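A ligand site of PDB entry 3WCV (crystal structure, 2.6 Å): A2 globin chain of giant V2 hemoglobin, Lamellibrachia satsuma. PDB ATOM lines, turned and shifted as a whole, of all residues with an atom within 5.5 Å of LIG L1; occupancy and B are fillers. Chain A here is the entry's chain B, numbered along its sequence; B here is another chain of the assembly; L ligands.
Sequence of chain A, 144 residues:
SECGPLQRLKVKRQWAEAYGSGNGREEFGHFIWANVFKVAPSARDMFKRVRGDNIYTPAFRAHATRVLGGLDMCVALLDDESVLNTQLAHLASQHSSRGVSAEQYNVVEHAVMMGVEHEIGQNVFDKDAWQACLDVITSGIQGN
NE2 of His 95 is bound to FE1 of LIG L1 (2.1 Å). The guanidinium group (NH2) of Arg 49 lies within salt-bridge range of an oxygen (O3) of LIG L1 (2.6 Å). An oxygen (O1) of LIG L1 lies within hydrogen-bond range of a ring nitrogen (NE2) of His 94 of chain B (2.8 Å). The side-chain amide nitrogen (NE2) of Gln 98 of chain B lies within hydrogen-bond range of an oxygen (O1) of LIG L1 (3.2 Å). A ring nitrogen (NE2) of His 63 is in hydrogen-bond range of an oxygen (O2) of LG2 L2, at 2.9 Å. O1 of LG3 L3 sits at hydrogen-bond distance from NE2 of Gln 94 of chain A (3.2 Å).
An iron atom (FE1) of LIG L1 is bound by an oxygen (O1) of LG2 L2, at 1.8 Å.
ND1 of His 95 lies within hydrogen-bond range of O of Leu 91, at 2.8 Å. The side-chain sulfur (SD) of Met 46 sits close to the side-chain amide oxygen (OE1) of Gln 104, at 3.6 Å. The guanidinium group (NE) of Arg 98 of chain A lies within hydrogen-bond range of the backbone carbonyl oxygen (O) of Gln 94 of chain A, at 3.0 Å. The side-chain sulfur (SG) of Cys 74 is in hydrogen-bond range of the backbone carbonyl oxygen (O) of Gly 70, 3.3 Å away.
Residues that only touch LIG L1: Met 46 (3.3 Å), Phe 47 (3.5 Å), Val 50 (3.5 Å), His 63 (3.7 Å), Arg 66 (3.4 Å), Val 67 (3.9 Å), Gly 70 (3.9 Å), Leu 71 (3.9 Å), Leu 91 (3.8 Å), Gln 94 of chain A (3.6 Å), Arg 98 of chain A (3.5 Å), Val 100 (3.5 Å), Gln 104 (3.5 Å), Tyr 105 (3.6 Å), Val 108 (3.4 Å) and Ile 141 (3.8 Å). Of the 26 residues printed, 20 come within 4 Å of LIG L1.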
ATOM      1  N   TRP A  33      17.822   7.737 -37.051  1.00  0.00           N
ATOM      2  CA  TRP A  33      18.207   8.994 -37.677  1.00  0.00           C
ATOM      3  C   TRP A  33      18.947   8.897 -39.007  1.00  0.00           C
ATOM      4  O   TRP A  33      19.027   9.878 -39.734  1.00  0.00           O
ATOM      5  CB  TRP A  33      19.003   9.840 -36.686  1.00  0.00           C
ATOM      6  CG  TRP A  33      18.132  10.441 -35.656  1.00  0.00           C
ATOM      7  CD1 TRP A  33      17.844   9.941 -34.423  1.00  0.00           C
ATOM      8  CD2 TRP A  33      17.360  11.634 -35.788  1.00  0.00           C
ATOM      9  NE1 TRP A  33      16.932  10.740 -33.781  1.00  0.00           N
ATOM     10  CE2 TRP A  33      16.618  11.787 -34.605  1.00  0.00           C
ATOM     11  CE3 TRP A  33      17.230  12.581 -36.805  1.00  0.00           C
ATOM     12  CZ2 TRP A  33      15.755  12.861 -34.394  1.00  0.00           C
ATOM     13  CZ3 TRP A  33      16.362  13.645 -36.603  1.00  0.00           C
ATOM     14  CH2 TRP A  33      15.642  13.777 -35.410  1.00  0.00           C
ATOM     15  N   ALA A  43      16.164  18.237 -43.841  1.00  0.00           N
ATOM     16  CA  ALA A  43      15.907  18.460 -42.412  1.00  0.00           C
ATOM     17  C   ALA A  43      17.128  18.634 -41.512  1.00  0.00           C
ATOM     18  O   ALA A  43      17.013  19.211 -40.418  1.00  0.00           O
ATOM     19  CB  ALA A  43      15.036  17.346 -41.871  1.00  0.00           C
ATOM     20  N   MET A  46      18.148  21.844 -39.477  1.00  0.00           N
ATOM     21  CA  MET A  46      17.559  22.281 -38.218  1.00  0.00           C
ATOM     22  C   MET A  46      18.369  21.809 -37.020  1.00  0.00           C
ATOM     23  O   MET A  46      18.120  22.227 -35.894  1.00  0.00           O
ATOM     24  CB  MET A  46      16.143  21.755 -38.094  1.00  0.00           C
ATOM     25  CG  MET A  46      15.161  22.375 -39.046  1.00  0.00           C
ATOM     26  SD  MET A  46      13.600  21.482 -38.970  1.00  0.00           S
ATOM     27  CE  MET A  46      13.227  21.673 -37.211  1.00  0.00           C
ATOM     28  N   PHE A  47      19.338  20.945 -37.270  1.00  0.00           N
ATOM     29  CA  PHE A  47      20.145  20.386 -36.210  1.00  0.00           C
ATOM     30  C   PHE A  47      21.580  20.904 -36.170  1.00  0.00           C
ATOM     31  O   PHE A  47      22.487  20.211 -35.686  1.00  0.00           O
ATOM     32  CB  PHE A  47      20.153  18.866 -36.349  1.00  0.00           C
ATOM     33  CG  PHE A  47      18.798  18.253 -36.231  1.00  0.00           C
ATOM     34  CD1 PHE A  47      18.248  18.009 -34.973  1.00  0.00           C
ATOM     35  CD2 PHE A  47      18.071  17.910 -37.367  1.00  0.00           C
ATOM     36  CE1 PHE A  47      16.999  17.432 -34.854  1.00  0.00           C
ATOM     37  CE2 PHE A  47      16.810  17.336 -37.255  1.00  0.00           C
ATOM     38  CZ  PHE A  47      16.271  17.090 -35.989  1.00  0.00           C
ATOM     39  N   ARG A  49      23.112  22.899 -34.236  1.00  0.00           N
ATOM     40  CA  ARG A  49      23.718  22.922 -32.903  1.00  0.00           C
ATOM     41  C   ARG A  49      24.131  21.555 -32.343  1.00  0.00           C
ATOM     42  O   ARG A  49      24.934  21.480 -31.411  1.00  0.00           O
ATOM     43  CB  ARG A  49      22.770  23.583 -31.906  1.00  0.00           C
ATOM     44  CG  ARG A  49      23.454  23.944 -30.589  1.00  0.00           C
ATOM     45  CD  ARG A  49      22.437  24.398 -29.588  1.00  0.00           C
ATOM     46  NE  ARG A  49      21.584  23.298 -29.160  1.00  0.00           N
ATOM     47  CZ  ARG A  49      21.975  22.358 -28.315  1.00  0.00           C
ATOM     48  NH1 ARG A  49      23.193  22.396 -27.799  1.00  0.00           N
ATOM     49  NH2 ARG A  49      21.138  21.386 -27.956  1.00  0.00           N
ATOM     50  N   VAL A  50      23.581  20.484 -32.909  1.00  0.00           N
ATOM     51  CA  VAL A  50      23.907  19.146 -32.432  1.00  0.00           C
ATOM     52  C   VAL A  50      24.565  18.325 -33.529  1.00  0.00           C
ATOM     53  O   VAL A  50      24.377  17.119 -33.608  1.00  0.00           O
ATOM     54  CB  VAL A  50      22.635  18.438 -31.906  1.00  0.00           C
ATOM     55  CG1 VAL A  50      21.981  19.301 -30.845  1.00  0.00           C
ATOM     56  CG2 VAL A  50      21.665  18.177 -33.039  1.00  0.00           C
ATOM     57  N   HIS A  63      21.957  13.941 -28.632  1.00  0.00           N
ATOM     58  CA  HIS A  63      20.649  14.432 -29.068  1.00  0.00           C
ATOM     59  C   HIS A  63      19.756  13.225 -29.321  1.00  0.00           C
ATOM     60  O   HIS A  63      18.654  13.133 -28.773  1.00  0.00           O
ATOM     61  CB  HIS A  63      20.780  15.264 -30.359  1.00  0.00           C
ATOM     62  CG  HIS A  63      19.477  15.495 -31.051  1.00  0.00           C
ATOM     63  ND1 HIS A  63      18.514  16.358 -30.572  1.00  0.00           N
ATOM     64  CD2 HIS A  63      18.944  14.923 -32.159  1.00  0.00           C
ATOM     65  CE1 HIS A  63      17.448  16.312 -31.352  1.00  0.00           C
ATOM     66  NE2 HIS A  63      17.687  15.449 -32.329  1.00  0.00           N
ATOM     67  N   ARG A  66      18.383  12.019 -26.286  1.00  0.00           N
ATOM     68  CA  ARG A  66      17.281  12.838 -25.782  1.00  0.00           C
ATOM     69  C   ARG A  66      15.981  12.582 -26.518  1.00  0.00           C
ATOM     70  O   ARG A  66      14.906  12.571 -25.905  1.00  0.00           O
ATOM     71  CB  ARG A  66      17.640  14.327 -25.856  1.00  0.00           C
ATOM     72  CG  ARG A  66      18.717  14.760 -24.876  1.00  0.00           C
ATOM     73  CD  ARG A  66      18.840  16.271 -24.823  1.00  0.00           C
ATOM     74  NE  ARG A  66      19.328  16.810 -26.087  1.00  0.00           N
ATOM     75  CZ  ARG A  66      20.606  16.855 -26.438  1.00  0.00           C
ATOM     76  NH1 ARG A  66      20.952  17.364 -27.625  1.00  0.00           N
ATOM     77  NH2 ARG A  66      21.541  16.424 -25.597  1.00  0.00           N
ATOM     78  N   VAL A  67      16.054  12.373 -27.827  1.00  0.00           N
ATOM     79  CA  VAL A  67      14.842  12.132 -28.595  1.00  0.00           C
ATOM     80  C   VAL A  67      14.179  10.824 -28.193  1.00  0.00           C
ATOM     81  O   VAL A  67      12.977  10.788 -27.925  1.00  0.00           O
ATOM     82  CB  VAL A  67      15.115  12.066 -30.110  1.00  0.00           C
ATOM     83  CG1 VAL A  67      13.842  11.660 -30.845  1.00  0.00           C
ATOM     84  CG2 VAL A  67      15.598  13.410 -30.618  1.00  0.00           C
ATOM     85  N   GLY A  70      12.560  10.883 -25.114  1.00  0.00           N
ATOM     86  CA  GLY A  70      11.280  11.557 -25.207  1.00  0.00           C
ATOM     87  C   GLY A  70      10.177  10.624 -25.660  1.00  0.00           C
ATOM     88  O   GLY A  70       9.030  10.712 -25.203  1.00  0.00           O
ATOM     89  N   LEU A  71      10.504   9.739 -26.596  1.00  0.00           N
ATOM     90  CA  LEU A  71       9.533   8.768 -27.103  1.00  0.00           C
ATOM     91  C   LEU A  71       9.181   7.808 -25.962  1.00  0.00           C
ATOM     92  O   LEU A  71       8.015   7.456 -25.765  1.00  0.00           O
ATOM     93  CB  LEU A  71      10.121   7.982 -28.267  1.00  0.00           C
ATOM     94  CG  LEU A  71       9.802   8.432 -29.688  1.00  0.00           C
ATOM     95  CD1 LEU A  71      10.611   7.610 -30.703  1.00  0.00           C
ATOM     96  CD2 LEU A  71       8.311   8.262 -29.925  1.00  0.00           C
ATOM     97  N   CYS A  74       6.650   9.146 -23.571  1.00  0.00           N
ATOM     98  CA  CYS A  74       5.318   9.116 -24.145  1.00  0.00           C
ATOM     99  C   CYS A  74       4.779   7.710 -24.203  1.00  0.00           C
ATOM    100  O   CYS A  74       3.629   7.499 -23.844  1.00  0.00           O
ATOM    101  CB  CYS A  74       5.299   9.708 -25.562  1.00  0.00           C
ATOM    102  SG  CYS A  74       5.887  11.395 -25.675  1.00  0.00           S
ATOM    103  N   LEU A  91       6.929  18.679 -24.756  1.00  0.00           N
ATOM    104  CA  LEU A  91       7.654  18.424 -25.987  1.00  0.00           C
ATOM    105  C   LEU A  91       7.273  19.489 -27.003  1.00  0.00           C
ATOM    106  O   LEU A  91       8.129  19.997 -27.739  1.00  0.00           O
ATOM    107  CB  LEU A  91       7.320  17.029 -26.534  1.00  0.00           C
ATOM    108  CG  LEU A  91       8.000  15.851 -25.826  1.00  0.00           C
ATOM    109  CD1 LEU A  91       7.409  14.530 -26.323  1.00  0.00           C
ATOM    110  CD2 LEU A  91       9.499  15.908 -26.070  1.00  0.00           C
ATOM    111  N   GLN A  94       9.151  22.546 -26.536  1.00  0.00           N
ATOM    112  CA  GLN A  94      10.571  22.411 -26.852  1.00  0.00           C
ATOM    113  C   GLN A  94      10.799  22.483 -28.358  1.00  0.00           C
ATOM    114  O   GLN A  94      11.932  22.680 -28.792  1.00  0.00           O
ATOM    115  CB  GLN A  94      11.114  21.079 -26.290  1.00  0.00           C
ATOM    116  CG  GLN A  94      11.072  20.978 -24.757  1.00  0.00           C
ATOM    117  CD  GLN A  94      11.595  19.646 -24.217  1.00  0.00           C
ATOM    118  OE1 GLN A  94      11.093  18.569 -24.582  1.00  0.00           O
ATOM    119  NE2 GLN A  94      12.596  19.705 -23.350  1.00  0.00           N
ATOM    120  N   HIS A  95       9.728  22.343 -29.133  1.00  0.00           N
ATOM    121  CA  HIS A  95       9.790  22.391 -30.589  1.00  0.00           C
ATOM    122  C   HIS A  95       9.075  23.593 -31.214  1.00  0.00           C
ATOM    123  O   HIS A  95       9.164  23.822 -32.414  1.00  0.00           O
ATOM    124  CB  HIS A  95       9.169  21.129 -31.198  1.00  0.00           C
ATOM    125  CG  HIS A  95       9.943  19.881 -30.932  1.00  0.00           C
ATOM    126  ND1 HIS A  95      10.087  19.347 -29.667  1.00  0.00           N
ATOM    127  CD2 HIS A  95      10.619  19.051 -31.765  1.00  0.00           C
ATOM    128  CE1 HIS A  95      10.807  18.248 -29.728  1.00  0.00           C
ATOM    129  NE2 HIS A  95      11.151  18.039 -30.987  1.00  0.00           N
ATOM    130  N   ARG A  98      10.868  26.190 -33.636  1.00  0.00           N
ATOM    131  CA  ARG A  98      11.729  25.531 -34.599  1.00  0.00           C
ATOM    132  C   ARG A  98      11.085  25.232 -35.947  1.00  0.00           C
ATOM    133  O   ARG A  98      11.732  24.783 -36.883  1.00  0.00           O
ATOM    134  CB  ARG A  98      12.285  24.244 -33.971  1.00  0.00           C
ATOM    135  CG  ARG A  98      13.036  24.506 -32.663  1.00  0.00           C
ATOM    136  CD  ARG A  98      13.472  23.218 -32.002  1.00  0.00           C
ATOM    137  NE  ARG A  98      14.085  23.440 -30.698  1.00  0.00           N
ATOM    138  CZ  ARG A  98      15.259  24.019 -30.502  1.00  0.00           C
ATOM    139  NH1 ARG A  98      15.710  24.176 -29.270  1.00  0.00           N
ATOM    140  NH2 ARG A  98      15.974  24.454 -31.535  1.00  0.00           N
ATOM    141  N   VAL A 100       8.712  22.881 -37.217  1.00  0.00           N
ATOM    142  CA  VAL A 100       8.745  21.519 -37.714  1.00  0.00           C
ATOM    143  C   VAL A 100       7.449  21.302 -38.473  1.00  0.00           C
ATOM    144  O   VAL A 100       6.370  21.629 -37.964  1.00  0.00           O
ATOM    145  CB  VAL A 100       8.839  20.501 -36.545  1.00  0.00           C
ATOM    146  CG1 VAL A 100       8.851  19.085 -37.096  1.00  0.00           C
ATOM    147  CG2 VAL A 100      10.083  20.775 -35.720  1.00  0.00           C
ATOM    148  N   GLN A 104       7.574  16.385 -41.588  1.00  0.00           N
ATOM    149  CA  GLN A 104       8.841  15.939 -41.023  1.00  0.00           C
ATOM    150  C   GLN A 104       8.477  15.032 -39.844  1.00  0.00           C
ATOM    151  O   GLN A 104       9.157  14.036 -39.584  1.00  0.00           O
ATOM    152  CB  GLN A 104       9.670  17.147 -40.548  1.00  0.00           C
ATOM    153  CG  GLN A 104      10.148  18.062 -41.665  1.00  0.00           C
ATOM    154  CD  GLN A 104      10.986  19.226 -41.148  1.00  0.00           C
ATOM    155  OE1 GLN A 104      10.560  19.970 -40.261  1.00  0.00           O
ATOM    156  NE2 GLN A 104      12.174  19.396 -41.716  1.00  0.00           N
ATOM    157  N   TYR A 105       7.385  15.362 -39.154  1.00  0.00           N
ATOM    158  CA  TYR A 105       6.928  14.535 -38.042  1.00  0.00           C
ATOM    159  C   TYR A 105       6.577  13.142 -38.561  1.00  0.00           C
ATOM    160  O   TYR A 105       6.889  12.140 -37.916  1.00  0.00           O
ATOM    161  CB  TYR A 105       5.707  15.153 -37.347  1.00  0.00           C
ATOM    162  CG  TYR A 105       6.043  16.161 -36.266  1.00  0.00           C
ATOM    163  CD1 TYR A 105       6.676  15.763 -35.094  1.00  0.00           C
ATOM    164  CD2 TYR A 105       5.763  17.517 -36.443  1.00  0.00           C
ATOM    165  CE1 TYR A 105       7.025  16.687 -34.107  1.00  0.00           C
ATOM    166  CE2 TYR A 105       6.105  18.455 -35.468  1.00  0.00           C
ATOM    167  CZ  TYR A 105       6.736  18.041 -34.300  1.00  0.00           C
ATOM    168  OH  TYR A 105       7.092  18.958 -33.342  1.00  0.00           O
ATOM    169  N   VAL A 108       9.919  11.062 -39.279  1.00  0.00           N
ATOM    170  CA  VAL A 108      10.458  10.511 -38.059  1.00  0.00           C
ATOM    171  C   VAL A 108       9.605   9.323 -37.603  1.00  0.00           C
ATOM    172  O   VAL A 108      10.116   8.339 -37.065  1.00  0.00           O
ATOM    173  CB  VAL A 108      10.519  11.600 -36.990  1.00  0.00           C
ATOM    174  CG1 VAL A 108      10.837  11.003 -35.632  1.00  0.00           C
ATOM    175  CG2 VAL A 108      11.577  12.614 -37.372  1.00  0.00           C
ATOM    176  N   VAL A 112      11.159   5.765 -36.933  1.00  0.00           N
ATOM    177  CA  VAL A 112      10.993   5.081 -35.659  1.00  0.00           C
ATOM    178  C   VAL A 112      10.398   3.685 -35.875  1.00  0.00           C
ATOM    179  O   VAL A 112      10.844   2.718 -35.263  1.00  0.00           O
ATOM    180  CB  VAL A 112      10.074   5.866 -34.711  1.00  0.00           C
ATOM    181  CG1 VAL A 112       9.643   4.981 -33.551  1.00  0.00           C
ATOM    182  CG2 VAL A 112      10.803   7.098 -34.184  1.00  0.00           C
ATOM    183  N   ILE A 137       0.983  10.641 -30.731  1.00  0.00           N
ATOM    184  CA  ILE A 137       2.116  11.295 -30.084  1.00  0.00           C
ATOM    185  C   ILE A 137       2.607  12.543 -30.781  1.00  0.00           C
ATOM    186  O   ILE A 137       2.800  13.576 -30.144  1.00  0.00           O
ATOM    187  CB  ILE A 137       3.288  10.302 -29.899  1.00  0.00           C
ATOM    188  CG1 ILE A 137       2.855   9.212 -28.906  1.00  0.00           C
ATOM    189  CG2 ILE A 137       4.535  11.030 -29.394  1.00  0.00           C
ATOM    190  CD1 ILE A 137       3.859   8.087 -28.720  1.00  0.00           C
ATOM    191  N   THR A 138       2.816  12.463 -32.092  1.00  0.00           N
ATOM    192  CA  THR A 138       3.286  13.618 -32.842  1.00  0.00           C
ATOM    193  C   THR A 138       2.174  14.651 -32.860  1.00  0.00           C
ATOM    194  O   THR A 138       2.413  15.841 -32.661  1.00  0.00           O
ATOM    195  CB  THR A 138       3.628  13.251 -34.295  1.00  0.00           C
ATOM    196  OG1 THR A 138       2.496  12.653 -34.925  1.00  0.00           O
ATOM    197  CG2 THR A 138       4.805  12.296 -34.320  1.00  0.00           C
ATOM    198  N   ILE A 141       2.393  16.731 -30.042  1.00  0.00           N
ATOM    199  CA  ILE A 141       3.602  17.542 -29.968  1.00  0.00           C
ATOM    200  C   ILE A 141       3.448  18.769 -30.864  1.00  0.00           C
ATOM    201  O   ILE A 141       4.141  19.773 -30.681  1.00  0.00           O
ATOM    202  CB  ILE A 141       4.862  16.755 -30.406  1.00  0.00           C
ATOM    203  CG1 ILE A 141       5.049  15.530 -29.509  1.00  0.00           C
ATOM    204  CG2 ILE A 141       6.091  17.650 -30.324  1.00  0.00           C
ATOM    205  CD1 ILE A 141       6.235  14.652 -29.864  1.00  0.00           C
ATOM    206  N   HIS B  94      24.500  19.223 -21.702  1.00  0.00           N
ATOM    207  CA  HIS B  94      23.175  19.675 -22.010  1.00  0.00           C
ATOM    208  C   HIS B  94      22.345  19.777 -20.723  1.00  0.00           C
ATOM    209  O   HIS B  94      21.607  20.737 -20.537  1.00  0.00           O
ATOM    210  CB  HIS B  94      22.510  18.708 -22.955  1.00  0.00           C
ATOM    211  CG  HIS B  94      21.182  19.164 -23.441  1.00  0.00           C
ATOM    212  ND1 HIS B  94      21.026  19.917 -24.580  1.00  0.00           N
ATOM    213  CD2 HIS B  94      19.928  18.946 -22.963  1.00  0.00           C
ATOM    214  CE1 HIS B  94      19.739  20.136 -24.793  1.00  0.00           C
ATOM    215  NE2 HIS B  94      19.056  19.556 -23.821  1.00  0.00           N
ATOM    216  N   GLN B  98      20.705  23.012 -18.593  1.00  0.00           N
ATOM    217  CA  GLN B  98      19.278  22.991 -18.263  1.00  0.00           C
ATOM    218  C   GLN B  98      19.064  23.330 -16.783  1.00  0.00           C
ATOM    219  O   GLN B  98      17.956  23.691 -16.383  1.00  0.00           O
ATOM    220  CB  GLN B  98      18.658  21.625 -18.596  1.00  0.00           C
ATOM    221  CG  GLN B  98      18.445  21.372 -20.099  1.00  0.00           C
ATOM    222  CD  GLN B  98      17.728  20.064 -20.373  1.00  0.00           C
ATOM    223  OE1 GLN B  98      18.098  19.021 -19.828  1.00  0.00           O
ATOM    224  NE2 GLN B  98      16.722  20.091 -21.232  1.00  0.00           N
HETATM  225  C1  LIG L   1      14.899  18.490 -29.836  1.00  0.00           C
HETATM  226  C2  LIG L   1      11.925  14.954 -28.890  1.00  0.00           C
HETATM  227  C3  LIG L   1      10.420  14.909 -33.475  1.00  0.00           C
HETATM  228  C4  LIG L   1      13.473  18.507 -34.408  1.00  0.00           C
HETATM  229  C5  LIG L   1      14.229  17.522 -29.164  1.00  0.00           C
HETATM  230  C6  LIG L   1      14.421  17.247 -27.793  1.00  0.00           C
HETATM  231  C7  LIG L   1      13.582  16.238 -27.514  1.00  0.00           C
HETATM  232  C8  LIG L   1      12.845  15.886 -28.722  1.00  0.00           C
HETATM  233  C9  LIG L   1      13.391  15.558 -26.153  1.00  0.00           C
HETATM  234  C10 LIG L   1      15.378  17.920 -26.838  1.00  0.00           C
HETATM  235  C11 LIG L   1      14.807  19.160 -26.202  1.00  0.00           C
HETATM  236  C12 LIG L   1      15.765  19.846 -25.230  1.00  0.00           C
HETATM  237  O1  LIG L   1      16.268  19.195 -24.280  1.00  0.00           O
HETATM  238  O2  LIG L   1      16.019  20.996 -25.425  1.00  0.00           O
HETATM  239  C13 LIG L   1      11.217  14.601 -30.048  1.00  0.00           C
HETATM  240  C14 LIG L   1      10.212  13.552 -30.110  1.00  0.00           C
HETATM  241  C15 LIG L   1       9.768  13.554 -31.471  1.00  0.00           C
HETATM  242  C16 LIG L   1      10.533  14.573 -32.117  1.00  0.00           C
HETATM  243  C17 LIG L   1       9.744  12.701 -28.988  1.00  0.00           C
HETATM  244  C18 LIG L   1       8.746  12.648 -31.953  1.00  0.00           C
HETATM  245  C19 LIG L   1       8.972  11.652 -32.782  1.00  0.00           C
HETATM  246  C20 LIG L   1      11.145  15.897 -34.121  1.00  0.00           C
HETATM  247  C21 LIG L   1      10.978  16.179 -35.547  1.00  0.00           C
HETATM  248  C22 LIG L   1      11.859  17.228 -35.869  1.00  0.00           C
HETATM  249  C23 LIG L   1      12.537  17.536 -34.548  1.00  0.00           C
HETATM  250  C24 LIG L   1      10.022  15.466 -36.503  1.00  0.00           C
HETATM  251  C25 LIG L   1      12.060  17.812 -37.067  1.00  0.00           C
HETATM  252  C26 LIG L   1      12.617  17.524 -38.192  1.00  0.00           C
HETATM  253  C27 LIG L   1      14.137  18.830 -33.228  1.00  0.00           C
HETATM  254  C28 LIG L   1      15.171  19.920 -33.115  1.00  0.00           C
HETATM  255  C29 LIG L   1      15.555  19.891 -31.803  1.00  0.00           C
HETATM  256  C30 LIG L   1      14.785  18.819 -31.152  1.00  0.00           C
HETATM  257  C31 LIG L   1      15.622  20.805 -34.252  1.00  0.00           C
HETATM  258  C32 LIG L   1      16.571  20.787 -31.129  1.00  0.00           C
HETATM  259  C33 LIG L   1      17.951  20.242 -31.118  1.00  0.00           C
HETATM  260  C34 LIG L   1      18.858  21.161 -30.420  1.00  0.00           C
HETATM  261  O3  LIG L   1      18.855  21.197 -29.163  1.00  0.00           O
HETATM  262  O4  LIG L   1      19.603  21.889 -31.077  1.00  0.00           O
HETATM  263  N1  LIG L   1      13.268  16.695 -29.752  1.00  0.00           N
HETATM  264  N2  LIG L   1      11.430  15.221 -31.225  1.00  0.00           N
HETATM  265  N3  LIG L   1      12.095  16.732 -33.567  1.00  0.00           N
HETATM  266  N4  LIG L   1      13.947  18.229 -32.040  1.00  0.00           N
HETATM  267 FE1  LIG L   1      12.691  16.727 -31.657  1.00  0.00          FE
HETATM  268  O1  LG2 L   2      13.987  15.653 -32.283  1.00  0.00           O
HETATM  269  O2  LG2 L   2      14.866  15.619 -33.160  1.00  0.00           O
HETATM  270  C1  LG3 L   3      14.640  20.260 -14.556  1.00  0.00           C
HETATM  271  C2  LG3 L   3      17.020  16.183 -14.371  1.00  0.00           C
HETATM  272  C3  LG3 L   3      18.714  17.307  -9.982  1.00  0.00           C
HETATM  273  C4  LG3 L   3      16.327  21.474 -10.237  1.00  0.00           C
HETATM  274  C5  LG3 L   3      15.134  19.052 -14.908  1.00  0.00           C
HETATM  275  C6  LG3 L   3      14.822  18.421 -16.129  1.00  0.00           C
HETATM  276  C7  LG3 L   3      15.511  17.253 -16.088  1.00  0.00           C
HETATM  277  C8  LG3 L   3      16.242  17.170 -14.821  1.00  0.00           C
HETATM  278  C9  LG3 L   3      15.536  16.156 -17.163  1.00  0.00           C
HETATM  279  C10 LG3 L   3      13.909  18.936 -17.249  1.00  0.00           C
HETATM  280  C11 LG3 L   3      14.635  19.655 -18.361  1.00  0.00           C
HETATM  281  C12 LG3 L   3      13.741  20.185 -19.507  1.00  0.00           C
HETATM  282  O1  LG3 L   3      13.048  19.374 -20.194  1.00  0.00           O
HETATM  283  O2  LG3 L   3      13.726  21.362 -19.718  1.00  0.00           O
HETATM  284  C13 LG3 L   3      17.714  16.094 -13.143  1.00  0.00           C
HETATM  285  C14 LG3 L   3      18.530  14.948 -12.742  1.00  0.00           C
HETATM  286  C15 LG3 L   3      19.027  15.290 -11.426  1.00  0.00           C
HETATM  287  C16 LG3 L   3      18.489  16.593 -11.151  1.00  0.00           C
HETATM  288  C17 LG3 L   3      18.770  13.712 -13.521  1.00  0.00           C
HETATM  289  C18 LG3 L   3      19.888  14.428 -10.635  1.00  0.00           C
HETATM  290  C19 LG3 L   3      21.196  14.328 -10.760  1.00  0.00           C
HETATM  291  C20 LG3 L   3      18.204  18.557  -9.688  1.00  0.00           C
HETATM  292  C21 LG3 L   3      18.505  19.255  -8.412  1.00  0.00           C
HETATM  293  C22 LG3 L   3      17.823  20.494  -8.455  1.00  0.00           C
HETATM  294  C23 LG3 L   3      17.122  20.459  -9.800  1.00  0.00           C
HETATM  295  C24 LG3 L   3      19.401  18.728  -7.280  1.00  0.00           C
HETATM  296  C25 LG3 L   3      17.809  21.478  -7.508  1.00  0.00           C
HETATM  297  C26 LG3 L   3      17.608  21.636  -6.240  1.00  0.00           C
HETATM  298  C27 LG3 L   3      15.639  21.508 -11.454  1.00  0.00           C
HETATM  299  C28 LG3 L   3      14.742  22.661 -11.884  1.00  0.00           C
HETATM  300  C29 LG3 L   3      14.273  22.270 -13.108  1.00  0.00           C
HETATM  301  C30 LG3 L   3      14.876  20.960 -13.411  1.00  0.00           C
HETATM  302  C31 LG3 L   3      14.470  23.906 -11.075  1.00  0.00           C
HETATM  303  C32 LG3 L   3      13.319  23.016 -14.023  1.00  0.00           C
HETATM  304  C33 LG3 L   3      11.927  22.448 -13.812  1.00  0.00           C
HETATM  305  C34 LG3 L   3      10.877  23.040 -14.641  1.00  0.00           C
HETATM  306  O3  LG3 L   3      10.253  24.056 -14.234  1.00  0.00           O
HETATM  307  O4  LG3 L   3      10.603  22.517 -15.734  1.00  0.00           O
HETATM  308  N1  LG3 L   3      16.006  18.309 -14.095  1.00  0.00           N
HETATM  309  N2  LG3 L   3      17.671  17.072 -12.219  1.00  0.00           N
HETATM  310  N3  LG3 L   3      17.375  19.322 -10.481  1.00  0.00           N
HETATM  311  N4  LG3 L   3      15.676  20.544 -12.390  1.00  0.00           N
HETATM  312 FE1  LG3 L   3      16.697  18.817 -12.299  1.00  0.00          FE
